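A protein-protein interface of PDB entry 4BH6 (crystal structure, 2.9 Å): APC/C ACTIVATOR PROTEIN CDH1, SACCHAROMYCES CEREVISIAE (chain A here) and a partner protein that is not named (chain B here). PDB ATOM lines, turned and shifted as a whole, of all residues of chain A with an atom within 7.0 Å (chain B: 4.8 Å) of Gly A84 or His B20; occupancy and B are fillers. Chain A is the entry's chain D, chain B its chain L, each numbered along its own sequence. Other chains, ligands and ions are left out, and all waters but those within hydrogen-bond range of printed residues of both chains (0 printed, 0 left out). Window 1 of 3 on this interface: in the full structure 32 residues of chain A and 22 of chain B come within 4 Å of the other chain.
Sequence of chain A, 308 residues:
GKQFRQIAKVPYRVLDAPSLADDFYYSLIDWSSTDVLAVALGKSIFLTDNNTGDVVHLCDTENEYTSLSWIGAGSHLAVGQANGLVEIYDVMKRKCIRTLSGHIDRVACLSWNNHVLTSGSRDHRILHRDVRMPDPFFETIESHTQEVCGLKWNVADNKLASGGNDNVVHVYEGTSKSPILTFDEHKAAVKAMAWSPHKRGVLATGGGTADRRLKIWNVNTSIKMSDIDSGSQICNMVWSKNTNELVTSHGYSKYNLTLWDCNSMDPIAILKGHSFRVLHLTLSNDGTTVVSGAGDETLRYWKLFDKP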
ATOM      1  N   ASN A  63      25.208 -14.232  21.729  1.00  0.00           N
ATOM      2  CA  ASN A  63      24.325 -13.168  22.115  1.00  0.00           C
ATOM      3  C   ASN A  63      23.042 -13.753  22.708  1.00  0.00           C
ATOM      4  O   ASN A  63      23.084 -14.503  23.687  1.00  0.00           O
ATOM      5  CB  ASN A  63      24.019 -12.357  20.853  1.00  0.00           C
ATOM      6  CG  ASN A  63      23.702 -10.920  21.138  1.00  0.00           C
ATOM      7  OD1 ASN A  63      22.703 -10.397  20.660  1.00  0.00           O
ATOM      8  ND2 ASN A  63      24.555 -10.268  21.911  1.00  0.00           N
ATOM      9  N   GLY A  80      16.541 -12.191  14.382  1.00  0.00           N
ATOM     10  CA  GLY A  80      17.124 -11.015  15.026  1.00  0.00           C
ATOM     11  C   GLY A  80      17.811 -11.322  16.346  1.00  0.00           C
ATOM     12  O   GLY A  80      17.503 -12.335  16.996  1.00  0.00           O
ATOM     13  N   GLN A  81      18.740 -10.452  16.743  1.00  0.00           N
ATOM     14  CA  GLN A  81      19.493 -10.643  17.979  1.00  0.00           C
ATOM     15  C   GLN A  81      19.451  -9.446  18.908  1.00  0.00           C
ATOM     16  O   GLN A  81      19.135  -8.325  18.467  1.00  0.00           O
ATOM     17  CB  GLN A  81      20.935 -10.956  17.666  1.00  0.00           C
ATOM     18  CG  GLN A  81      21.117 -12.406  17.344  1.00  0.00           C
ATOM     19  CD  GLN A  81      22.464 -12.684  16.775  1.00  0.00           C
ATOM     20  OE1 GLN A  81      23.470 -12.641  17.481  1.00  0.00           O
ATOM     21  NE2 GLN A  81      22.499 -12.971  15.484  1.00  0.00           N
ATOM     22  N   ALA A  82      19.798  -9.685  20.181  1.00  0.00           N
ATOM     23  CA  ALA A  82      19.848  -8.622  21.180  1.00  0.00           C
ATOM     24  C   ALA A  82      20.793  -7.463  20.778  1.00  0.00           C
ATOM     25  O   ALA A  82      20.537  -6.313  21.124  1.00  0.00           O
ATOM     26  CB  ALA A  82      20.173  -9.171  22.560  1.00  0.00           C
ATOM     27  N   ASN A  83      21.846  -7.751  20.016  1.00  0.00           N
ATOM     28  CA  ASN A  83      22.764  -6.700  19.592  1.00  0.00           C
ATOM     29  C   ASN A  83      22.375  -5.976  18.296  1.00  0.00           C
ATOM     30  O   ASN A  83      23.208  -5.239  17.734  1.00  0.00           O
ATOM     31  CB  ASN A  83      24.178  -7.239  19.450  1.00  0.00           C
ATOM     32  CG  ASN A  83      24.298  -8.296  18.360  1.00  0.00           C
ATOM     33  OD1 ASN A  83      23.368  -8.532  17.587  1.00  0.00           O
ATOM     34  ND2 ASN A  83      25.448  -8.953  18.305  1.00  0.00           N
ATOM     35  N   GLY A  84      21.143  -6.201  17.823  1.00  0.00           N
ATOM     36  CA  GLY A  84      20.619  -5.497  16.638  1.00  0.00           C
ATOM     37  C   GLY A  84      20.871  -6.160  15.300  1.00  0.00           C
ATOM     38  O   GLY A  84      20.331  -5.732  14.266  1.00  0.00           O
ATOM     39  N   LEU A  85      21.680  -7.213  15.314  1.00  0.00           N
ATOM     40  CA  LEU A  85      21.999  -7.944  14.103  1.00  0.00           C
ATOM     41  C   LEU A  85      20.784  -8.707  13.590  1.00  0.00           C
ATOM     42  O   LEU A  85      20.010  -9.253  14.386  1.00  0.00           O
ATOM     43  CB  LEU A  85      23.140  -8.905  14.390  1.00  0.00           C
ATOM     44  CG  LEU A  85      24.133  -9.207  13.269  1.00  0.00           C
ATOM     45  CD1 LEU A  85      24.858  -7.939  12.816  1.00  0.00           C
ATOM     46  CD2 LEU A  85      25.111 -10.306  13.701  1.00  0.00           C
ATOM     47  N   VAL A  86      20.583  -8.725  12.272  1.00  0.00           N
ATOM     48  CA  VAL A  86      19.524  -9.548  11.667  1.00  0.00           C
ATOM     49  C   VAL A  86      20.159 -10.452  10.621  1.00  0.00           C
ATOM     50  O   VAL A  86      20.916  -9.985   9.785  1.00  0.00           O
ATOM     51  CB  VAL A  86      18.408  -8.710  11.009  1.00  0.00           C
ATOM     52  CG1 VAL A  86      17.258  -9.599  10.531  1.00  0.00           C
ATOM     53  CG2 VAL A  86      17.913  -7.647  11.975  1.00  0.00           C
ATOM     54  N   THR A  99      23.725 -11.455   6.415  1.00  0.00           N
ATOM     55  CA  THR A  99      23.949 -10.833   7.705  1.00  0.00           C
ATOM     56  C   THR A  99      23.678  -9.341   7.556  1.00  0.00           C
ATOM     57  O   THR A  99      24.441  -8.640   6.888  1.00  0.00           O
ATOM     58  CB  THR A  99      25.423 -11.058   8.144  1.00  0.00           C
ATOM     59  OG1 THR A  99      25.739 -12.461   8.160  1.00  0.00           O
ATOM     60  CG2 THR A  99      25.693 -10.484   9.520  1.00  0.00           C
ATOM     61  N   LEU A 100      22.583  -8.862   8.154  1.00  0.00           N
ATOM     62  CA  LEU A 100      22.100  -7.493   7.938  1.00  0.00           C
ATOM     63  C   LEU A 100      22.299  -6.607   9.154  1.00  0.00           C
ATOM     64  O   LEU A 100      21.752  -6.887  10.237  1.00  0.00           O
ATOM     65  CB  LEU A 100      20.609  -7.477   7.584  1.00  0.00           C
ATOM     66  CG  LEU A 100      19.995  -7.932   6.257  1.00  0.00           C
ATOM     67  CD1 LEU A 100      20.992  -7.829   5.121  1.00  0.00           C
ATOM     68  CD2 LEU A 100      19.355  -9.316   6.368  1.00  0.00           C
ATOM     69  N   SER A 101      23.038  -5.513   8.961  1.00  0.00           N
ATOM     70  CA  SER A 101      23.212  -4.511  10.011  1.00  0.00           C
ATOM     71  C   SER A 101      22.212  -3.381   9.853  1.00  0.00           C
ATOM     72  O   SER A 101      21.304  -3.471   9.034  1.00  0.00           O
ATOM     73  CB  SER A 101      24.579  -3.908   9.930  1.00  0.00           C
ATOM     74  OG  SER A 101      24.557  -2.921   8.917  1.00  0.00           O
ATOM     75  N   GLY A 102      22.397  -2.311  10.627  1.00  0.00           N
ATOM     76  CA  GLY A 102      21.458  -1.190  10.631  1.00  0.00           C
ATOM     77  C   GLY A 102      20.960  -0.848  12.024  1.00  0.00           C
ATOM     78  O   GLY A 102      20.836   0.335  12.359  1.00  0.00           O
ATOM     79  N   HIS A 103      20.656  -1.870  12.830  1.00  0.00           N
ATOM     80  CA  HIS A 103      20.148  -1.612  14.162  1.00  0.00           C
ATOM     81  C   HIS A 103      21.260  -1.563  15.154  1.00  0.00           C
ATOM     82  O   HIS A 103      22.262  -2.245  14.994  1.00  0.00           O
ATOM     83  CB  HIS A 103      19.141  -2.651  14.581  1.00  0.00           C
ATOM     84  CG  HIS A 103      17.841  -2.513  13.877  1.00  0.00           C
ATOM     85  ND1 HIS A 103      17.059  -1.386  13.993  1.00  0.00           N
ATOM     86  CD2 HIS A 103      17.189  -3.343  13.029  1.00  0.00           C
ATOM     87  CE1 HIS A 103      15.975  -1.527  13.248  1.00  0.00           C
ATOM     88  NE2 HIS A 103      16.033  -2.706  12.651  1.00  0.00           N
ATOM     89  N   ILE A 104      21.072  -0.750  16.184  1.00  0.00           N
ATOM     90  CA  ILE A 104      22.103  -0.538  17.171  1.00  0.00           C
ATOM     91  C   ILE A 104      21.645  -1.022  18.539  1.00  0.00           C
ATOM     92  O   ILE A 104      22.265  -0.714  19.541  1.00  0.00           O
ATOM     93  CB  ILE A 104      22.542   0.944  17.219  1.00  0.00           C
ATOM     94  CG1 ILE A 104      21.397   1.851  17.686  1.00  0.00           C
ATOM     95  CG2 ILE A 104      23.038   1.385  15.854  1.00  0.00           C
ATOM     96  CD1 ILE A 104      21.854   3.240  18.089  1.00  0.00           C
ATOM     97  N   ASP A 105      20.550  -1.768  18.563  1.00  0.00           N
ATOM     98  CA  ASP A 105      19.985  -2.326  19.791  1.00  0.00           C
ATOM     99  C   ASP A 105      18.996  -3.398  19.385  1.00  0.00           C
ATOM    100  O   ASP A 105      18.552  -3.418  18.242  1.00  0.00           O
ATOM    101  CB  ASP A 105      19.265  -1.251  20.600  1.00  0.00           C
ATOM    102  CG  ASP A 105      19.041  -1.649  22.052  1.00  0.00           C
ATOM    103  OD1 ASP A 105      19.415  -2.774  22.407  1.00  0.00           O
ATOM    104  OD2 ASP A 105      18.492  -0.839  22.842  1.00  0.00           O
ATOM    105  N   ARG A 106      18.643  -4.277  20.318  1.00  0.00           N
ATOM    106  CA  ARG A 106      17.883  -5.507  20.009  1.00  0.00           C
ATOM    107  C   ARG A 106      16.712  -5.362  19.027  1.00  0.00           C
ATOM    108  O   ARG A 106      16.004  -4.378  19.027  1.00  0.00           O
ATOM    109  CB  ARG A 106      17.410  -6.224  21.285  1.00  0.00           C
ATOM    110  CG  ARG A 106      16.439  -5.430  22.104  1.00  0.00           C
ATOM    111  CD  ARG A 106      15.498  -6.341  22.869  1.00  0.00           C
ATOM    112  NE  ARG A 106      14.520  -5.537  23.611  1.00  0.00           N
ATOM    113  CZ  ARG A 106      14.019  -5.893  24.780  1.00  0.00           C
ATOM    114  NH1 ARG A 106      14.380  -7.041  25.324  1.00  0.00           N
ATOM    115  NH2 ARG A 106      13.144  -5.122  25.384  1.00  0.00           N
ATOM    116  N   VAL A 107      16.541  -6.374  18.193  1.00  0.00           N
ATOM    117  CA  VAL A 107      15.492  -6.430  17.194  1.00  0.00           C
ATOM    118  C   VAL A 107      14.467  -7.413  17.710  1.00  0.00           C
ATOM    119  O   VAL A 107      14.650  -8.618  17.601  1.00  0.00           O
ATOM    120  CB  VAL A 107      16.058  -6.892  15.841  1.00  0.00           C
ATOM    121  CG1 VAL A 107      14.960  -7.075  14.814  1.00  0.00           C
ATOM    122  CG2 VAL A 107      17.111  -5.897  15.363  1.00  0.00           C
ATOM    123  N   SER A 119      12.449  -4.925   9.921  1.00  0.00           N
ATOM    124  CA  SER A 119      12.795  -5.130  11.309  1.00  0.00           C
ATOM    125  C   SER A 119      12.516  -3.907  12.154  1.00  0.00           C
ATOM    126  O   SER A 119      12.624  -2.791  11.683  1.00  0.00           O
ATOM    127  CB  SER A 119      14.248  -5.533  11.443  1.00  0.00           C
ATOM    128  OG  SER A 119      15.067  -4.539  10.877  1.00  0.00           O
ATOM    129  N   SER A 121      13.185  -2.334  16.291  1.00  0.00           N
ATOM    130  CA  SER A 121      14.214  -2.464  17.315  1.00  0.00           C
ATOM    131  C   SER A 121      13.960  -1.572  18.531  1.00  0.00           C
ATOM    132  O   SER A 121      13.099  -0.684  18.507  1.00  0.00           O
ATOM    133  CB  SER A 121      15.575  -2.117  16.697  1.00  0.00           C
ATOM    134  OG  SER A 121      16.557  -1.854  17.679  1.00  0.00           O
ATOM    135  N   ASP A 123      16.352   0.451  19.591  1.00  0.00           N
ATOM    136  CA  ASP A 123      16.592   1.808  19.067  1.00  0.00           C
ATOM    137  C   ASP A 123      15.208   2.151  18.587  1.00  0.00           C
ATOM    138  O   ASP A 123      14.310   1.295  18.705  1.00  0.00           O
ATOM    139  CB  ASP A 123      17.668   1.876  17.973  1.00  0.00           C
ATOM    140  CG  ASP A 123      17.316   1.108  16.706  1.00  0.00           C
ATOM    141  OD1 ASP A 123      16.131   1.077  16.305  1.00  0.00           O
ATOM    142  OD2 ASP A 123      18.263   0.572  16.074  1.00  0.00           O
ATOM    143  N   ARG A 129      13.995  -3.690   4.163  1.00  0.00           N
ATOM    144  CA  ARG A 129      15.158  -4.299   3.523  1.00  0.00           C
ATOM    145  C   ARG A 129      14.788  -5.101   2.283  1.00  0.00           C
ATOM    146  O   ARG A 129      13.993  -6.055   2.361  1.00  0.00           O
ATOM    147  CB  ARG A 129      15.853  -5.223   4.508  1.00  0.00           C
ATOM    148  CG  ARG A 129      16.142  -4.608   5.865  1.00  0.00           C
ATOM    149  CD  ARG A 129      16.692  -5.657   6.804  1.00  0.00           C
ATOM    150  NE  ARG A 129      16.785  -5.169   8.175  1.00  0.00           N
ATOM    151  CZ  ARG A 129      17.870  -4.606   8.694  1.00  0.00           C
ATOM    152  NH1 ARG A 129      18.965  -4.450   7.969  1.00  0.00           N
ATOM    153  NH2 ARG A 129      17.865  -4.211   9.958  1.00  0.00           N
ATOM    154  N   ALA B  16      30.298  -6.927   7.002  1.00  0.00           N
ATOM    155  CA  ALA B  16      29.023  -6.494   7.580  1.00  0.00           C
ATOM    156  C   ALA B  16      29.048  -6.581   9.080  1.00  0.00           C
ATOM    157  O   ALA B  16      28.675  -5.624   9.746  1.00  0.00           O
ATOM    158  CB  ALA B  16      27.874  -7.304   7.030  1.00  0.00           C
ATOM    159  N   VAL B  17      29.505  -7.722   9.598  1.00  0.00           N
ATOM    160  CA  VAL B  17      29.584  -7.975  11.032  1.00  0.00           C
ATOM    161  C   VAL B  17      30.431  -6.909  11.711  1.00  0.00           C
ATOM    162  O   VAL B  17      29.992  -6.268  12.668  1.00  0.00           O
ATOM    163  CB  VAL B  17      30.148  -9.388  11.324  1.00  0.00           C
ATOM    164  CG1 VAL B  17      30.472  -9.562  12.807  1.00  0.00           C
ATOM    165  CG2 VAL B  17      29.149 -10.449  10.887  1.00  0.00           C
ATOM    166  N   HIS B  18      31.636  -6.718  11.179  1.00  0.00           N
ATOM    167  CA  HIS B  18      32.626  -5.785  11.720  1.00  0.00           C
ATOM    168  C   HIS B  18      32.085  -4.348  11.796  1.00  0.00           C
ATOM    169  O   HIS B  18      32.202  -3.678  12.824  1.00  0.00           O
ATOM    170  CB  HIS B  18      33.904  -5.861  10.874  1.00  0.00           C
ATOM    171  CG  HIS B  18      35.113  -5.249  11.517  1.00  0.00           C
ATOM    172  ND1 HIS B  18      35.405  -3.905  11.421  1.00  0.00           N
ATOM    173  CD2 HIS B  18      36.127  -5.803  12.228  1.00  0.00           C
ATOM    174  CE1 HIS B  18      36.535  -3.653  12.062  1.00  0.00           C
ATOM    175  NE2 HIS B  18      36.997  -4.788  12.557  1.00  0.00           N
ATOM    176  N   ARG B  19      31.467  -3.885  10.713  1.00  0.00           N
ATOM    177  CA  ARG B  19      30.944  -2.529  10.667  1.00  0.00           C
ATOM    178  C   ARG B  19      29.840  -2.345  11.693  1.00  0.00           C
ATOM    179  O   ARG B  19      29.815  -1.354  12.433  1.00  0.00           O
ATOM    180  CB  ARG B  19      30.406  -2.196   9.280  1.00  0.00           C
ATOM    181  CG  ARG B  19      30.280  -0.693   9.044  1.00  0.00           C
ATOM    182  CD  ARG B  19      29.260  -0.312   7.961  1.00  0.00           C
ATOM    183  NE  ARG B  19      29.447  -1.014   6.675  1.00  0.00           N
ATOM    184  CZ  ARG B  19      30.467  -0.851   5.815  1.00  0.00           C
ATOM    185  NH1 ARG B  19      31.462   0.003   6.069  1.00  0.00           N
ATOM    186  NH2 ARG B  19      30.501  -1.564   4.688  1.00  0.00           N
ATOM    187  N   HIS B  20      28.934  -3.313  11.721  1.00  0.00           N
ATOM    188  CA  HIS B  20      27.849  -3.330  12.669  1.00  0.00           C
ATOM    189  C   HIS B  20      28.346  -3.214  14.101  1.00  0.00           C
ATOM    190  O   HIS B  20      27.869  -2.366  14.872  1.00  0.00           O
ATOM    191  CB  HIS B  20      27.040  -4.614  12.515  1.00  0.00           C
ATOM    192  CG  HIS B  20      25.865  -4.696  13.439  1.00  0.00           C
ATOM    193  ND1 HIS B  20      25.904  -5.387  14.630  1.00  0.00           N
ATOM    194  CD2 HIS B  20      24.627  -4.151  13.357  1.00  0.00           C
ATOM    195  CE1 HIS B  20      24.737  -5.274  15.238  1.00  0.00           C
ATOM    196  NE2 HIS B  20      23.946  -4.528  14.487  1.00  0.00           N
ATOM    197  N   ASN B  21      29.303  -4.069  14.452  1.00  0.00           N
ATOM    198  CA  ASN B  21      29.863  -4.079  15.795  1.00  0.00           C
ATOM    199  C   ASN B  21      30.451  -2.741  16.211  1.00  0.00           C
ATOM    200  O   ASN B  21      30.401  -2.369  17.376  1.00  0.00           O
ATOM    201  CB  ASN B  21      30.859  -5.231  15.976  1.00  0.00           C
ATOM    202  CG  ASN B  21      30.160  -6.573  16.126  1.00  0.00           C
ATOM    203  OD1 ASN B  21      29.027  -6.644  16.622  1.00  0.00           O
ATOM    204  ND2 ASN B  21      30.820  -7.644  15.696  1.00  0.00           N
ATOM    205  N   GLU B  22      30.973  -1.996  15.255  1.00  0.00           N
ATOM    206  CA  GLU B  22      31.517  -0.709  15.598  1.00  0.00           C
ATOM    207  C   GLU B  22      30.450   0.365  15.691  1.00  0.00           C
ATOM    208  O   GLU B  22      30.450   1.171  16.627  1.00  0.00           O
ATOM    209  CB  GLU B  22      32.634  -0.340  14.652  1.00  0.00           C
ATOM    210  CG  GLU B  22      33.902  -1.100  15.012  1.00  0.00           C
ATOM    211  CD  GLU B  22      34.939  -1.005  13.935  1.00  0.00           C
ATOM    212  OE1 GLU B  22      34.553  -0.647  12.794  1.00  0.00           O
ATOM    213  OE2 GLU B  22      36.123  -1.283  14.238  1.00  0.00           O
ATOM    214  N   ILE B  23      29.521   0.358  14.743  1.00  0.00           N
ATOM    215  CA  ILE B  23      28.356   1.232  14.834  1.00  0.00           C
ATOM    216  C   ILE B  23      27.635   1.013  16.159  1.00  0.00           C
ATOM    217  O   ILE B  23      27.279   1.970  16.841  1.00  0.00           O
ATOM    218  CB  ILE B  23      27.420   1.050  13.627  1.00  0.00           C
ATOM    219  CG1 ILE B  23      28.093   1.682  12.404  1.00  0.00           C
ATOM    220  CG2 ILE B  23      26.056   1.672  13.895  1.00  0.00           C
ATOM    221  CD1 ILE B  23      27.564   1.248  11.051  1.00  0.00           C
ATOM    222  N   TYR B  24      27.471  -0.249  16.533  1.00  0.00           N
ATOM    223  CA  TYR B  24      26.786  -0.619  17.771  1.00  0.00           C
ATOM    224  C   TYR B  24      27.517  -0.187  19.053  1.00  0.00           C
ATOM    225  O   TYR B  24      26.895   0.330  19.989  1.00  0.00           O
ATOM    226  CB  TYR B  24      26.496  -2.133  17.778  1.00  0.00           C
ATOM    227  CG  TYR B  24      25.993  -2.689  19.097  1.00  0.00           C
ATOM    228  CD1 TYR B  24      24.633  -2.733  19.390  1.00  0.00           C
ATOM    229  CD2 TYR B  24      26.886  -3.186  20.047  1.00  0.00           C
ATOM    230  CE1 TYR B  24      24.184  -3.240  20.596  1.00  0.00           C
ATOM    231  CE2 TYR B  24      26.442  -3.699  21.246  1.00  0.00           C
ATOM    232  CZ  TYR B  24      25.095  -3.716  21.518  1.00  0.00           C
ATOM    233  OH  TYR B  24      24.665  -4.223  22.717  1.00  0.00           O
ATOM    234  N   ASN B  25      28.825  -0.398  19.093  1.00  0.00           N
ATOM    235  CA  ASN B  25      29.586  -0.086  20.296  1.00  0.00           C
ATOM    236  C   ASN B  25      29.845   1.405  20.484  1.00  0.00           C
ATOM    237  O   ASN B  25      30.183   1.853  21.577  1.00  0.00           O
ATOM    238  CB  ASN B  25      30.873  -0.907  20.355  1.00  0.00           C
ATOM    239  CG  ASN B  25      30.612  -2.364  20.734  1.00  0.00           C
ATOM    240  OD1 ASN B  25      30.201  -2.678  21.862  1.00  0.00           O
ATOM    241  ND2 ASN B  25      30.845  -3.263  19.785  1.00  0.00           N
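Printed residues of chain A that touch a printed residue of chain B: Asn A83, Gly A84, Leu A85, Thr A99, Ser A101, Gly A102, His A103 and Ile A104. Hydrophobic or aromatic side chains of chain A within 4 Å of the printed part of chain B: Leu A85 and Ile A104. Along chain B the printed residues that touch a printed residue of chain A span positions 16 to 24. Among the printed residues, 11 pairs touch across the chains. Among the printed residues, no Asp or Glu carboxylate lies within 4 Å of a Lys or Arg side-chain nitrogen of the other chain.
NE2 of His B20 lies close to O of Asn A83 (3.4 Å). The backbone carbonyl oxygen of His A103 lies within hydrogen-bond range of a ring nitrogen (NE2) of His B20.
Among the printed residues, merely in contact across the chains: Asn A83 with Tyr B24 (3.3 Å), Gly A84 with His B20 (3.6 Å), Leu A85 with His B20 (3.3 Å), Thr A99 with Ala B16 (3.7 Å), Thr A99 with Val B17 (3.7 Å), Ser A101 with His B20 (3.4 Å), Gly A102 with His B20 (3.98 Å), Ile A104 with Ile B23 (3.6 Å) and Ile A104 with Tyr B24 (3.1 Å).
Gly A84 touches just one residue of chain B: His B20 (3.6 Å). Of the printed residues of chain A, Ile B23 touches Ile A104 (3.6 Å). Of the printed residues of chain B, Ser A101 touches His B20 (3.4 Å). Ala A82 touches none of the printed residues of chain B. The nearest printed residue of chain B that does not touch Gly A84 is Tyr B24 (5.1 Å). The nearest printed residue of chain B that does not touch Ser A101 is Ala B16 (4.4 Å).
OD1 of Asn A63 sits at hydrogen-bond distance from N of Asn A83 (2.9 Å). OD1 of Asn A83 is in hydrogen-bond range of N of Leu A85. A ring nitrogen (NE2) of His A103 sits at hydrogen-bond distance from the side-chain hydroxyl (OG) of Ser A119 (2.7 Å). A ring nitrogen (ND1) of His A103 is in hydrogen-bond range of the side-chain carboxylate (OD2) of Asp A123. OD2 of Asp A123 lies within hydrogen-bond range of N of Ile A104 (3.1 Å). The backbone carbonyl oxygen (O) of Val B17 is in hydrogen-bond range of the side-chain amide nitrogen (ND2) of Asn B21 (3.4 Å).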
